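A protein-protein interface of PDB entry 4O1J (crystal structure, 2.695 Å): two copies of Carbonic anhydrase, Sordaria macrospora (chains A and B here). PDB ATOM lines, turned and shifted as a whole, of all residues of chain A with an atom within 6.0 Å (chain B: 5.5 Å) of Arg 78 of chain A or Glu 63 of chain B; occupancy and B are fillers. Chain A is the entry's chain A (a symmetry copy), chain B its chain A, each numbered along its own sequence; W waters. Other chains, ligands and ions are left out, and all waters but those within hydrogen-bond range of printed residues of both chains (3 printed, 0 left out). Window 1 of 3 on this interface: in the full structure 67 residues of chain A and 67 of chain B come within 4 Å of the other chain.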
ATOM      1  N   TRP A  53     -19.865   8.229  30.054  1.00  0.00           N
ATOM      2  CA  TRP A  53     -19.722   9.036  28.855  1.00  0.00           C
ATOM      3  C   TRP A  53     -20.261   8.269  27.652  1.00  0.00           C
ATOM      4  O   TRP A  53     -19.833   7.152  27.393  1.00  0.00           O
ATOM      5  CB  TRP A  53     -18.247   9.408  28.666  1.00  0.00           C
ATOM      6  CG  TRP A  53     -17.897  10.089  27.383  1.00  0.00           C
ATOM      7  CD1 TRP A  53     -17.689   9.499  26.170  1.00  0.00           C
ATOM      8  CD2 TRP A  53     -17.674  11.488  27.190  1.00  0.00           C
ATOM      9  NE1 TRP A  53     -17.364  10.447  25.228  1.00  0.00           N
ATOM     10  CE2 TRP A  53     -17.349  11.682  25.833  1.00  0.00           C
ATOM     11  CE3 TRP A  53     -17.725  12.606  28.033  1.00  0.00           C
ATOM     12  CZ2 TRP A  53     -17.071  12.941  25.300  1.00  0.00           C
ATOM     13  CZ3 TRP A  53     -17.456  13.858  27.502  1.00  0.00           C
ATOM     14  CH2 TRP A  53     -17.131  14.014  26.150  1.00  0.00           C
ATOM     15  N   ILE A  54     -21.221   8.845  26.936  1.00  0.00           N
ATOM     16  CA  ILE A  54     -21.666   8.257  25.676  1.00  0.00           C
ATOM     17  C   ILE A  54     -21.283   9.187  24.542  1.00  0.00           C
ATOM     18  O   ILE A  54     -21.789  10.309  24.446  1.00  0.00           O
ATOM     19  CB  ILE A  54     -23.192   7.993  25.633  1.00  0.00           C
ATOM     20  CG1 ILE A  54     -23.613   7.035  26.752  1.00  0.00           C
ATOM     21  CG2 ILE A  54     -23.581   7.384  24.298  1.00  0.00           C
ATOM     22  CD1 ILE A  54     -25.123   6.854  26.886  1.00  0.00           C
ATOM     23  N   GLY A  55     -20.371   8.728  23.693  1.00  0.00           N
ATOM     24  CA  GLY A  55     -19.889   9.570  22.616  1.00  0.00           C
ATOM     25  C   GLY A  55     -19.695   8.918  21.262  1.00  0.00           C
ATOM     26  O   GLY A  55     -19.964   7.721  21.053  1.00  0.00           O
ATOM     27  N   CYS A  56     -19.216   9.734  20.327  1.00  0.00           N
ATOM     28  CA  CYS A  56     -18.963   9.273  18.973  1.00  0.00           C
ATOM     29  C   CYS A  56     -17.624   8.557  18.911  1.00  0.00           C
ATOM     30  O   CYS A  56     -16.672   8.952  19.568  1.00  0.00           O
ATOM     31  CB  CYS A  56     -18.998  10.437  17.979  1.00  0.00           C
ATOM     32  SG  CYS A  56     -18.974   9.919  16.234  1.00  0.00           S
ATOM     33  N   SER A  57     -17.567   7.518  18.089  1.00  0.00           N
ATOM     34  CA  SER A  57     -16.381   6.695  17.899  1.00  0.00           C
ATOM     35  C   SER A  57     -15.203   7.480  17.335  1.00  0.00           C
ATOM     36  O   SER A  57     -14.064   7.009  17.384  1.00  0.00           O
ATOM     37  CB  SER A  57     -16.715   5.530  16.956  1.00  0.00           C
ATOM     38  OG  SER A  57     -17.423   4.505  17.632  1.00  0.00           O
ATOM     39  N   ASP A  58     -15.502   8.678  16.826  1.00  0.00           N
ATOM     40  CA  ASP A  58     -14.540   9.611  16.237  1.00  0.00           C
ATOM     41  C   ASP A  58     -13.192   9.598  16.953  1.00  0.00           C
ATOM     42  O   ASP A  58     -13.127   9.648  18.187  1.00  0.00           O
ATOM     43  CB  ASP A  58     -15.132  11.024  16.267  1.00  0.00           C
ATOM     44  CG  ASP A  58     -14.505  11.955  15.245  1.00  0.00           C
ATOM     45  OD1 ASP A  58     -13.355  12.400  15.468  1.00  0.00           O
ATOM     46  OD2 ASP A  58     -15.173  12.257  14.226  1.00  0.00           O
ATOM     47  N   SER A  59     -12.116   9.523  16.174  1.00  0.00           N
ATOM     48  CA  SER A  59     -10.776   9.419  16.745  1.00  0.00           C
ATOM     49  C   SER A  59     -10.390  10.701  17.482  1.00  0.00           C
ATOM     50  O   SER A  59      -9.505  10.702  18.342  1.00  0.00           O
ATOM     51  CB  SER A  59      -9.740   9.100  15.654  1.00  0.00           C
ATOM     52  OG  SER A  59      -9.731  10.073  14.619  1.00  0.00           O
ATOM     53  N   ARG A  60     -11.080  11.787  17.160  1.00  0.00           N
ATOM     54  CA  ARG A  60     -10.753  13.079  17.727  1.00  0.00           C
ATOM     55  C   ARG A  60     -11.495  13.334  19.042  1.00  0.00           C
ATOM     56  O   ARG A  60     -11.376  14.405  19.635  1.00  0.00           O
ATOM     57  CB  ARG A  60     -11.066  14.167  16.708  1.00  0.00           C
ATOM     58  CG  ARG A  60     -10.419  13.910  15.358  1.00  0.00           C
ATOM     59  CD  ARG A  60     -10.969  14.837  14.300  1.00  0.00           C
ATOM     60  NE  ARG A  60     -12.318  14.457  13.894  1.00  0.00           N
ATOM     61  CZ  ARG A  60     -13.080  15.166  13.065  1.00  0.00           C
ATOM     62  NH1 ARG A  60     -12.633  16.307  12.553  1.00  0.00           N
ATOM     63  NH2 ARG A  60     -14.299  14.739  12.758  1.00  0.00           N
ATOM     64  N   CYS A  61     -12.240  12.341  19.517  1.00  0.00           N
ATOM     65  CA  CYS A  61     -13.031  12.525  20.732  1.00  0.00           C
ATOM     66  C   CYS A  61     -12.757  11.542  21.878  1.00  0.00           C
ATOM     67  O   CYS A  61     -13.706  10.958  22.403  1.00  0.00           O
ATOM     68  CB  CYS A  61     -14.516  12.442  20.382  1.00  0.00           C
ATOM     69  SG  CYS A  61     -15.083  13.661  19.178  1.00  0.00           S
ATOM     70  N   PRO A  62     -11.482  11.359  22.286  1.00  0.00           N
ATOM     71  CA  PRO A  62     -11.256  10.473  23.440  1.00  0.00           C
ATOM     72  C   PRO A  62     -11.600  11.148  24.766  1.00  0.00           C
ATOM     73  O   PRO A  62     -10.889  12.044  25.213  1.00  0.00           O
ATOM     74  CB  PRO A  62      -9.763  10.165  23.358  1.00  0.00           C
ATOM     75  CG  PRO A  62      -9.179  11.358  22.688  1.00  0.00           C
ATOM     76  CD  PRO A  62     -10.215  11.862  21.726  1.00  0.00           C
ATOM     77  N   GLU A  63     -12.675  10.691  25.393  1.00  0.00           N
ATOM     78  CA  GLU A  63     -13.249  11.341  26.574  1.00  0.00           C
ATOM     79  C   GLU A  63     -12.236  11.645  27.683  1.00  0.00           C
ATOM     80  O   GLU A  63     -12.286  12.710  28.290  1.00  0.00           O
ATOM     81  CB  GLU A  63     -14.399  10.483  27.141  1.00  0.00           C
ATOM     82  CG  GLU A  63     -13.973   9.211  27.857  1.00  0.00           C
ATOM     83  CD  GLU A  63     -13.129   8.307  26.995  1.00  0.00           C
ATOM     84  OE1 GLU A  63     -13.483   8.133  25.810  1.00  0.00           O
ATOM     85  OE2 GLU A  63     -12.090   7.806  27.485  1.00  0.00           O
ATOM     86  N   VAL A  76     -17.131   4.434  29.673  1.00  0.00           N
ATOM     87  CA  VAL A  76     -17.584   4.984  28.390  1.00  0.00           C
ATOM     88  C   VAL A  76     -18.154   3.981  27.381  1.00  0.00           C
ATOM     89  O   VAL A  76     -17.710   2.838  27.273  1.00  0.00           O
ATOM     90  CB  VAL A  76     -16.429   5.796  27.689  1.00  0.00           C
ATOM     91  CG1 VAL A  76     -15.164   5.771  28.515  1.00  0.00           C
ATOM     92  CG2 VAL A  76     -16.138   5.304  26.274  1.00  0.00           C
ATOM     93  N   HIS A  77     -19.169   4.448  26.659  1.00  0.00           N
ATOM     94  CA  HIS A  77     -19.672   3.787  25.471  1.00  0.00           C
ATOM     95  C   HIS A  77     -19.520   4.739  24.289  1.00  0.00           C
ATOM     96  O   HIS A  77     -19.851   5.929  24.373  1.00  0.00           O
ATOM     97  CB  HIS A  77     -21.134   3.367  25.650  1.00  0.00           C
ATOM     98  CG  HIS A  77     -21.769   2.831  24.402  1.00  0.00           C
ATOM     99  ND1 HIS A  77     -21.367   1.658  23.804  1.00  0.00           N
ATOM    100  CD2 HIS A  77     -22.791   3.305  23.648  1.00  0.00           C
ATOM    101  CE1 HIS A  77     -22.105   1.434  22.731  1.00  0.00           C
ATOM    102  NE2 HIS A  77     -22.976   2.420  22.616  1.00  0.00           N
ATOM    103  N   ARG A  78     -19.007   4.208  23.189  1.00  0.00           N
ATOM    104  CA  ARG A  78     -18.813   4.994  21.983  1.00  0.00           C
ATOM    105  C   ARG A  78     -19.290   4.244  20.758  1.00  0.00           C
ATOM    106  O   ARG A  78     -18.967   3.068  20.565  1.00  0.00           O
ATOM    107  CB  ARG A  78     -17.346   5.384  21.800  1.00  0.00           C
ATOM    108  CG  ARG A  78     -16.850   6.492  22.704  1.00  0.00           C
ATOM    109  CD  ARG A  78     -15.917   7.377  21.912  1.00  0.00           C
ATOM    110  NE  ARG A  78     -14.527   7.298  22.340  1.00  0.00           N
ATOM    111  CZ  ARG A  78     -13.499   7.726  21.612  1.00  0.00           C
ATOM    112  NH1 ARG A  78     -13.695   8.239  20.404  1.00  0.00           N
ATOM    113  NH2 ARG A  78     -12.268   7.627  22.091  1.00  0.00           N
ATOM    114  N   ASN A  79     -20.082   4.924  19.943  1.00  0.00           N
ATOM    115  CA  ASN A  79     -20.517   4.348  18.678  1.00  0.00           C
ATOM    116  C   ASN A  79     -20.540   5.400  17.580  1.00  0.00           C
ATOM    117  O   ASN A  79     -20.140   6.543  17.796  1.00  0.00           O
ATOM    118  CB  ASN A  79     -21.892   3.697  18.822  1.00  0.00           C
ATOM    119  CG  ASN A  79     -22.957   4.670  19.289  1.00  0.00           C
ATOM    120  OD1 ASN A  79     -23.245   5.674  18.627  1.00  0.00           O
ATOM    121  ND2 ASN A  79     -23.577   4.358  20.420  1.00  0.00           N
ATOM    122  N   ILE A  80     -21.007   5.013  16.399  1.00  0.00           N
ATOM    123  CA  ILE A  80     -21.104   5.955  15.295  1.00  0.00           C
ATOM    124  C   ILE A  80     -22.105   7.069  15.594  1.00  0.00           C
ATOM    125  O   ILE A  80     -23.285   6.808  15.815  1.00  0.00           O
ATOM    126  CB  ILE A  80     -21.494   5.247  13.992  1.00  0.00           C
ATOM    127  CG1 ILE A  80     -20.393   4.264  13.595  1.00  0.00           C
ATOM    128  CG2 ILE A  80     -21.717   6.264  12.876  1.00  0.00           C
ATOM    129  CD1 ILE A  80     -19.016   4.900  13.448  1.00  0.00           C
ATOM    130  N   TRP B  53      -9.999   0.608  17.573  1.00  0.00           N
ATOM    131  CA  TRP B  53      -9.879  -0.025  18.874  1.00  0.00           C
ATOM    132  C   TRP B  53     -11.247  -0.514  19.337  1.00  0.00           C
ATOM    133  O   TRP B  53     -12.190   0.263  19.396  1.00  0.00           O
ATOM    134  CB  TRP B  53      -9.275   0.972  19.870  1.00  0.00           C
ATOM    135  CG  TRP B  53      -9.246   0.541  21.301  1.00  0.00           C
ATOM    136  CD1 TRP B  53     -10.276   0.589  22.195  1.00  0.00           C
ATOM    137  CD2 TRP B  53      -8.118   0.031  22.018  1.00  0.00           C
ATOM    138  NE1 TRP B  53      -9.863   0.127  23.422  1.00  0.00           N
ATOM    139  CE2 TRP B  53      -8.537  -0.224  23.338  1.00  0.00           C
ATOM    140  CE3 TRP B  53      -6.789  -0.244  21.671  1.00  0.00           C
ATOM    141  CZ2 TRP B  53      -7.678  -0.734  24.313  1.00  0.00           C
ATOM    142  CZ3 TRP B  53      -5.938  -0.758  22.637  1.00  0.00           C
ATOM    143  CH2 TRP B  53      -6.385  -0.995  23.941  1.00  0.00           C
ATOM    144  N   CYS B  61      -9.744   1.687  31.169  1.00  0.00           N
ATOM    145  CA  CYS B  61      -9.203   1.339  29.857  1.00  0.00           C
ATOM    146  C   CYS B  61      -9.388   2.381  28.746  1.00  0.00           C
ATOM    147  O   CYS B  61      -9.864   2.025  27.668  1.00  0.00           O
ATOM    148  CB  CYS B  61      -9.833   0.029  29.386  1.00  0.00           C
ATOM    149  SG  CYS B  61      -9.558  -1.383  30.477  1.00  0.00           S
ATOM    150  N   PRO B  62      -9.005   3.655  28.980  1.00  0.00           N
ATOM    151  CA  PRO B  62      -9.117   4.616  27.871  1.00  0.00           C
ATOM    152  C   PRO B  62      -7.997   4.454  26.846  1.00  0.00           C
ATOM    153  O   PRO B  62      -6.847   4.783  27.122  1.00  0.00           O
ATOM    154  CB  PRO B  62      -9.023   5.970  28.569  1.00  0.00           C
ATOM    155  CG  PRO B  62      -8.205   5.700  29.783  1.00  0.00           C
ATOM    156  CD  PRO B  62      -8.530   4.301  30.218  1.00  0.00           C
ATOM    157  N   GLU B  63      -8.351   3.968  25.664  1.00  0.00           N
ATOM    158  CA  GLU B  63      -7.383   3.578  24.637  1.00  0.00           C
ATOM    159  C   GLU B  63      -6.321   4.641  24.333  1.00  0.00           C
ATOM    160  O   GLU B  63      -5.152   4.314  24.161  1.00  0.00           O
ATOM    161  CB  GLU B  63      -8.119   3.193  23.337  1.00  0.00           C
ATOM    162  CG  GLU B  63      -8.715   4.354  22.556  1.00  0.00           C
ATOM    163  CD  GLU B  63      -9.668   5.187  23.375  1.00  0.00           C
ATOM    164  OE1 GLU B  63     -10.485   4.588  24.105  1.00  0.00           O
ATOM    165  OE2 GLU B  63      -9.572   6.435  23.325  1.00  0.00           O
ATOM    166  N   THR B  64      -6.728   5.902  24.270  1.00  0.00           N
ATOM    167  CA  THR B  64      -5.843   6.953  23.799  1.00  0.00           C
ATOM    168  C   THR B  64      -4.814   7.319  24.857  1.00  0.00           C
ATOM    169  O   THR B  64      -3.696   7.724  24.528  1.00  0.00           O
ATOM    170  CB  THR B  64      -6.641   8.198  23.386  1.00  0.00           C
ATOM    171  OG1 THR B  64      -7.676   7.809  22.475  1.00  0.00           O
ATOM    172  CG2 THR B  64      -5.748   9.198  22.690  1.00  0.00           C
ATOM    173  N   THR B  65      -5.180   7.157  26.125  1.00  0.00           N
ATOM    174  CA  THR B  65      -4.252   7.427  27.223  1.00  0.00           C
ATOM    175  C   THR B  65      -3.236   6.300  27.390  1.00  0.00           C
ATOM    176  O   THR B  65      -2.027   6.547  27.444  1.00  0.00           O
ATOM    177  CB  THR B  65      -4.988   7.629  28.570  1.00  0.00           C
ATOM    178  OG1 THR B  65      -5.861   8.759  28.482  1.00  0.00           O
ATOM    179  CG2 THR B  65      -3.989   7.888  29.685  1.00  0.00           C
ATOM    180  N   ILE B  66      -3.728   5.064  27.451  1.00  0.00           N
ATOM    181  CA  ILE B  66      -2.872   3.923  27.750  1.00  0.00           C
ATOM    182  C   ILE B  66      -1.961   3.566  26.585  1.00  0.00           C
ATOM    183  O   ILE B  66      -0.932   2.920  26.776  1.00  0.00           O
ATOM    184  CB  ILE B  66      -3.710   2.687  28.141  1.00  0.00           C
ATOM    185  CG1 ILE B  66      -4.585   2.238  26.967  1.00  0.00           C
ATOM    186  CG2 ILE B  66      -4.561   2.990  29.362  1.00  0.00           C
ATOM    187  CD1 ILE B  66      -5.418   1.009  27.247  1.00  0.00           C
ATOM    188  N   LEU B  67      -2.313   4.024  25.390  1.00  0.00           N
ATOM    189  CA  LEU B  67      -1.461   3.821  24.224  1.00  0.00           C
ATOM    190  C   LEU B  67      -0.532   5.016  24.052  1.00  0.00           C
ATOM    191  O   LEU B  67       0.323   5.029  23.163  1.00  0.00           O
ATOM    192  CB  LEU B  67      -2.297   3.620  22.961  1.00  0.00           C
ATOM    193  CG  LEU B  67      -3.106   2.333  22.821  1.00  0.00           C
ATOM    194  CD1 LEU B  67      -3.904   2.363  21.534  1.00  0.00           C
ATOM    195  CD2 LEU B  67      -2.197   1.120  22.857  1.00  0.00           C
ATOM    196  N   GLY B  68      -0.707   6.018  24.909  1.00  0.00           N
ATOM    197  CA  GLY B  68       0.117   7.211  24.880  1.00  0.00           C
ATOM    198  C   GLY B  68       0.088   7.901  23.531  1.00  0.00           C
ATOM    199  O   GLY B  68       1.129   8.323  23.019  1.00  0.00           O
ATOM    200  N   VAL B  74      -6.871   7.257  17.004  1.00  0.00           N
ATOM    201  CA  VAL B  74      -7.558   6.016  17.370  1.00  0.00           C
ATOM    202  C   VAL B  74      -9.091   6.142  17.306  1.00  0.00           C
ATOM    203  O   VAL B  74      -9.701   6.878  18.080  1.00  0.00           O
ATOM    204  CB  VAL B  74      -7.156   5.534  18.772  1.00  0.00           C
ATOM    205  CG1 VAL B  74      -7.903   4.267  19.116  1.00  0.00           C
ATOM    206  CG2 VAL B  74      -5.656   5.294  18.847  1.00  0.00           C
ATOM    207  N   VAL B  76     -12.625   4.474  17.996  1.00  0.00           N
ATOM    208  CA  VAL B  76     -12.914   3.435  18.990  1.00  0.00           C
ATOM    209  C   VAL B  76     -14.392   3.089  19.205  1.00  0.00           C
ATOM    210  O   VAL B  76     -15.280   3.940  19.141  1.00  0.00           O
ATOM    211  CB  VAL B  76     -12.280   3.802  20.387  1.00  0.00           C
ATOM    212  CG1 VAL B  76     -11.565   5.132  20.329  1.00  0.00           C
ATOM    213  CG2 VAL B  76     -13.307   3.809  21.516  1.00  0.00           C
ATOM    214  N   HIS B  77     -14.624   1.800  19.443  1.00  0.00           N
ATOM    215  CA  HIS B  77     -15.888   1.298  19.945  1.00  0.00           C
ATOM    216  C   HIS B  77     -15.635   0.612  21.284  1.00  0.00           C
ATOM    217  O   HIS B  77     -14.691  -0.174  21.438  1.00  0.00           O
ATOM    218  CB  HIS B  77     -16.532   0.330  18.949  1.00  0.00           C
ATOM    219  CG  HIS B  77     -17.755  -0.358  19.475  1.00  0.00           C
ATOM    220  ND1 HIS B  77     -18.918   0.314  19.777  1.00  0.00           N
ATOM    221  CD2 HIS B  77     -17.998  -1.666  19.738  1.00  0.00           C
ATOM    222  CE1 HIS B  77     -19.823  -0.545  20.214  1.00  0.00           C
ATOM    223  NE2 HIS B  77     -19.288  -1.753  20.197  1.00  0.00           N
ATOM    224  N   ARG B  78     -16.480   0.924  22.255  1.00  0.00           N
ATOM    225  CA  ARG B  78     -16.367   0.340  23.580  1.00  0.00           C
ATOM    226  C   ARG B  78     -17.716  -0.113  24.097  1.00  0.00           C
ATOM    227  O   ARG B  78     -18.703   0.626  24.032  1.00  0.00           O
ATOM    228  CB  ARG B  78     -15.748   1.324  24.573  1.00  0.00           C
ATOM    229  CG  ARG B  78     -14.254   1.528  24.442  1.00  0.00           C
ATOM    230  CD  ARG B  78     -13.662   1.648  25.826  1.00  0.00           C
ATOM    231  NE  ARG B  78     -13.153   2.977  26.135  1.00  0.00           N
ATOM    232  CZ  ARG B  78     -12.885   3.404  27.366  1.00  0.00           C
ATOM    233  NH1 ARG B  78     -13.101   2.619  28.413  1.00  0.00           N
ATOM    234  NH2 ARG B  78     -12.410   4.627  27.549  1.00  0.00           N
ATOM    235  N   ASN B  90     -24.753  -2.225  16.246  1.00  0.00           N
ATOM    236  CA  ASN B  90     -23.987  -1.145  16.856  1.00  0.00           C
ATOM    237  C   ASN B  90     -22.490  -1.270  16.552  1.00  0.00           C
ATOM    238  O   ASN B  90     -21.866  -0.323  16.067  1.00  0.00           O
ATOM    239  CB  ASN B  90     -24.226  -1.133  18.370  1.00  0.00           C
ATOM    240  CG  ASN B  90     -23.670   0.107  19.050  1.00  0.00           C
ATOM    241  OD1 ASN B  90     -22.609   0.616  18.684  1.00  0.00           O
ATOM    242  ND2 ASN B  90     -24.377   0.582  20.071  1.00  0.00           N
ATOM    243  N   VAL B  94     -19.601   0.599  13.525  1.00  0.00           N
ATOM    244  CA  VAL B  94     -18.299   1.194  13.807  1.00  0.00           C
ATOM    245  C   VAL B  94     -17.237   0.525  12.953  1.00  0.00           C
ATOM    246  O   VAL B  94     -16.382   1.196  12.372  1.00  0.00           O
ATOM    247  CB  VAL B  94     -17.902   1.069  15.300  1.00  0.00           C
ATOM    248  CG1 VAL B  94     -16.516   1.632  15.520  1.00  0.00           C
ATOM    249  CG2 VAL B  94     -18.914   1.778  16.192  1.00  0.00           C
HETATM  250  O   HOH W   1     -10.565   8.666  20.391  1.00  0.00           O
HETATM  251  O   HOH W   2      -7.277   8.810  19.532  1.00  0.00           O
HETATM  252  O   HOH W   3     -22.292   2.237  15.966  1.00  0.00           O
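Water W3 lies within hydrogen-bond range of the backbone carbonyl oxygen (O) of Asn 90 of chain B (2.6 Å) and the backbone NH (N) of Ile 80 of chain A (3.1 Å). Water W1 lies within hydrogen-bond range of the guanidinium group of Arg 78 of chain A (2.6 Å), the backbone carbonyl oxygen of Val 74 of chain B (3.0 Å) and the backbone carbonyl oxygen of Ser 59 of chain A (3.1 Å). Water W2 lies within hydrogen-bond range of the backbone NH (N) of Val 74 of chain B (3.0 Å), the side-chain hydroxyl (OG1) of Thr 64 of chain B (3.1 Å) and the backbone carbonyl oxygen (O) of Ser 59 of chain A (3.2 Å).
O of Cys 61 of chain B sits close to NH1 of Arg 78 of chain B, at 3.4 Å. N of His 77 of chain A lies within hydrogen-bond range of O of Trp 53 of chain A, at 2.9 Å. O of Cys 56 of chain A sits close to NH1 of Arg 78 of chain A (3.2 Å). The backbone carbonyl oxygen (O) of Ser 57 of chain A sits at hydrogen-bond distance from the guanidinium group (NH1) of Arg 78 of chain A (3.3 Å). O of Cys 61 of chain A sits close to NH1 of Arg 78 of chain A (3.4 Å). A ring nitrogen (NE2) of His 77 of chain A sits at hydrogen-bond distance from the side-chain amide nitrogen of Asn 79 of chain A.
Printed residues of chain B within 4 Å of Ser 59 of chain A: Val 74. Arg 78 of chain A touches just these residues of chain B: Glu 63, Val 76, His 77 and Arg 78. Of the printed residues of chain A, Pro 62 of chain B touches Glu 63. Of chain A, only Pro 62 and Arg 78 come within 4 Å of Glu 63 of chain B. Of the printed residues of chain A, Val 74 of chain B touches Ser 59 (3.1 Å). Of the printed residues of chain A, His 77 of chain B touches His 77 and Arg 78. The nearest residue of chain B that does not touch Arg 78 of chain A is Val 94 of chain B (4.6 Å). The nearest residue of chain A that does not touch Glu 63 of chain B is Glu 63 of chain A (4.9 Å). The nearest printed residue of chain A that does not touch His 77 of chain B is Ser 57 of chain A (4.2 Å).
Val 74 of chain B touches Ser 59 of chain A (O to CA, 3.1 Å). CB of Pro 62 of chain A touches OE2 of Glu 63 of chain B, 3.7 Å away. Pro 62 of chain A touches Thr 64 of chain B. Glu 63 of chain A touches Pro 62 of chain B (OE2 to CB, 3.7 Å). NH2 of Arg 78 of chain B touches CG1 of Val 76 of chain A (3.1 Å). CE1 of His 77 of chain A touches CE1 of His 77 of chain B (3.9 Å). Arg 78 of chain A touches Val 76 of chain B (NH2 to CG1, 3.1 Å). O of Arg 78 of chain B touches N of Arg 78 of chain A (3.7 Å). Asn 79 of chain A touches Asn 90 of chain B. Asn 79 of chain A touches Val 94 of chain B (CA to CG2, 3.9 Å).
Of the 16 printed residues of chain A, 9 touch a printed residue of chain B. Among the printed residues, 18 pairs touch across the chains. Among the printed residues, Asp or Glu carboxylates within 4 Å of a Lys or Arg side-chain nitrogen of the other chain: Glu 63 of chain A with Arg 78 of chain B and Arg 78 of chain A with Glu 63 of chain B.
Pro 62 of chain A touches Glu 63 of chain B, and with the chains exchanged Glu 63 of chain A touches Pro 62 of chain B. Glu 63 of chain A touches Arg 78 of chain B, and with the chains exchanged Arg 78 of chain A touches Glu 63 of chain B. Val 76 of chain A touches Arg 78 of chain B, and with the chains exchanged Arg 78 of chain A touches Val 76 of chain B. His 77 of chain A touches Arg 78 of chain B, and with the chains exchanged Arg 78 of chain A touches His 77 of chain B. 7 positions are printed for both chains. Of the 18 pairs that touch across the chains among the printed residues, 10 have their exchanged pair printed and touching as well.
NH2 of Arg 78 of chain A lies within salt-bridge range of OE2 of Glu 63 of chain B (3.2 Å). The side-chain hydroxyl (OG) of Ser 57 of chain A sits at hydrogen-bond distance from the backbone carbonyl oxygen (O) of Val 76 of chain B (2.7 Å). O of Arg 78 of chain A sits at hydrogen-bond distance from ND1 of His 77 of chain B (2.9 Å). The guanidinium group (NH2) of Arg 78 of chain B lies within salt-bridge range of the side-chain carboxylate (OE2) of Glu 63 of chain A. The backbone carbonyl oxygen (O) of Arg 78 of chain B is in hydrogen-bond range of a ring nitrogen (ND1) of His 77 of chain A (2.9 Å). The side-chain amide nitrogen (ND2) of Asn 90 of chain B is in hydrogen-bond range of a ring nitrogen (NE2) of His 77 of chain A (3.4 Å).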
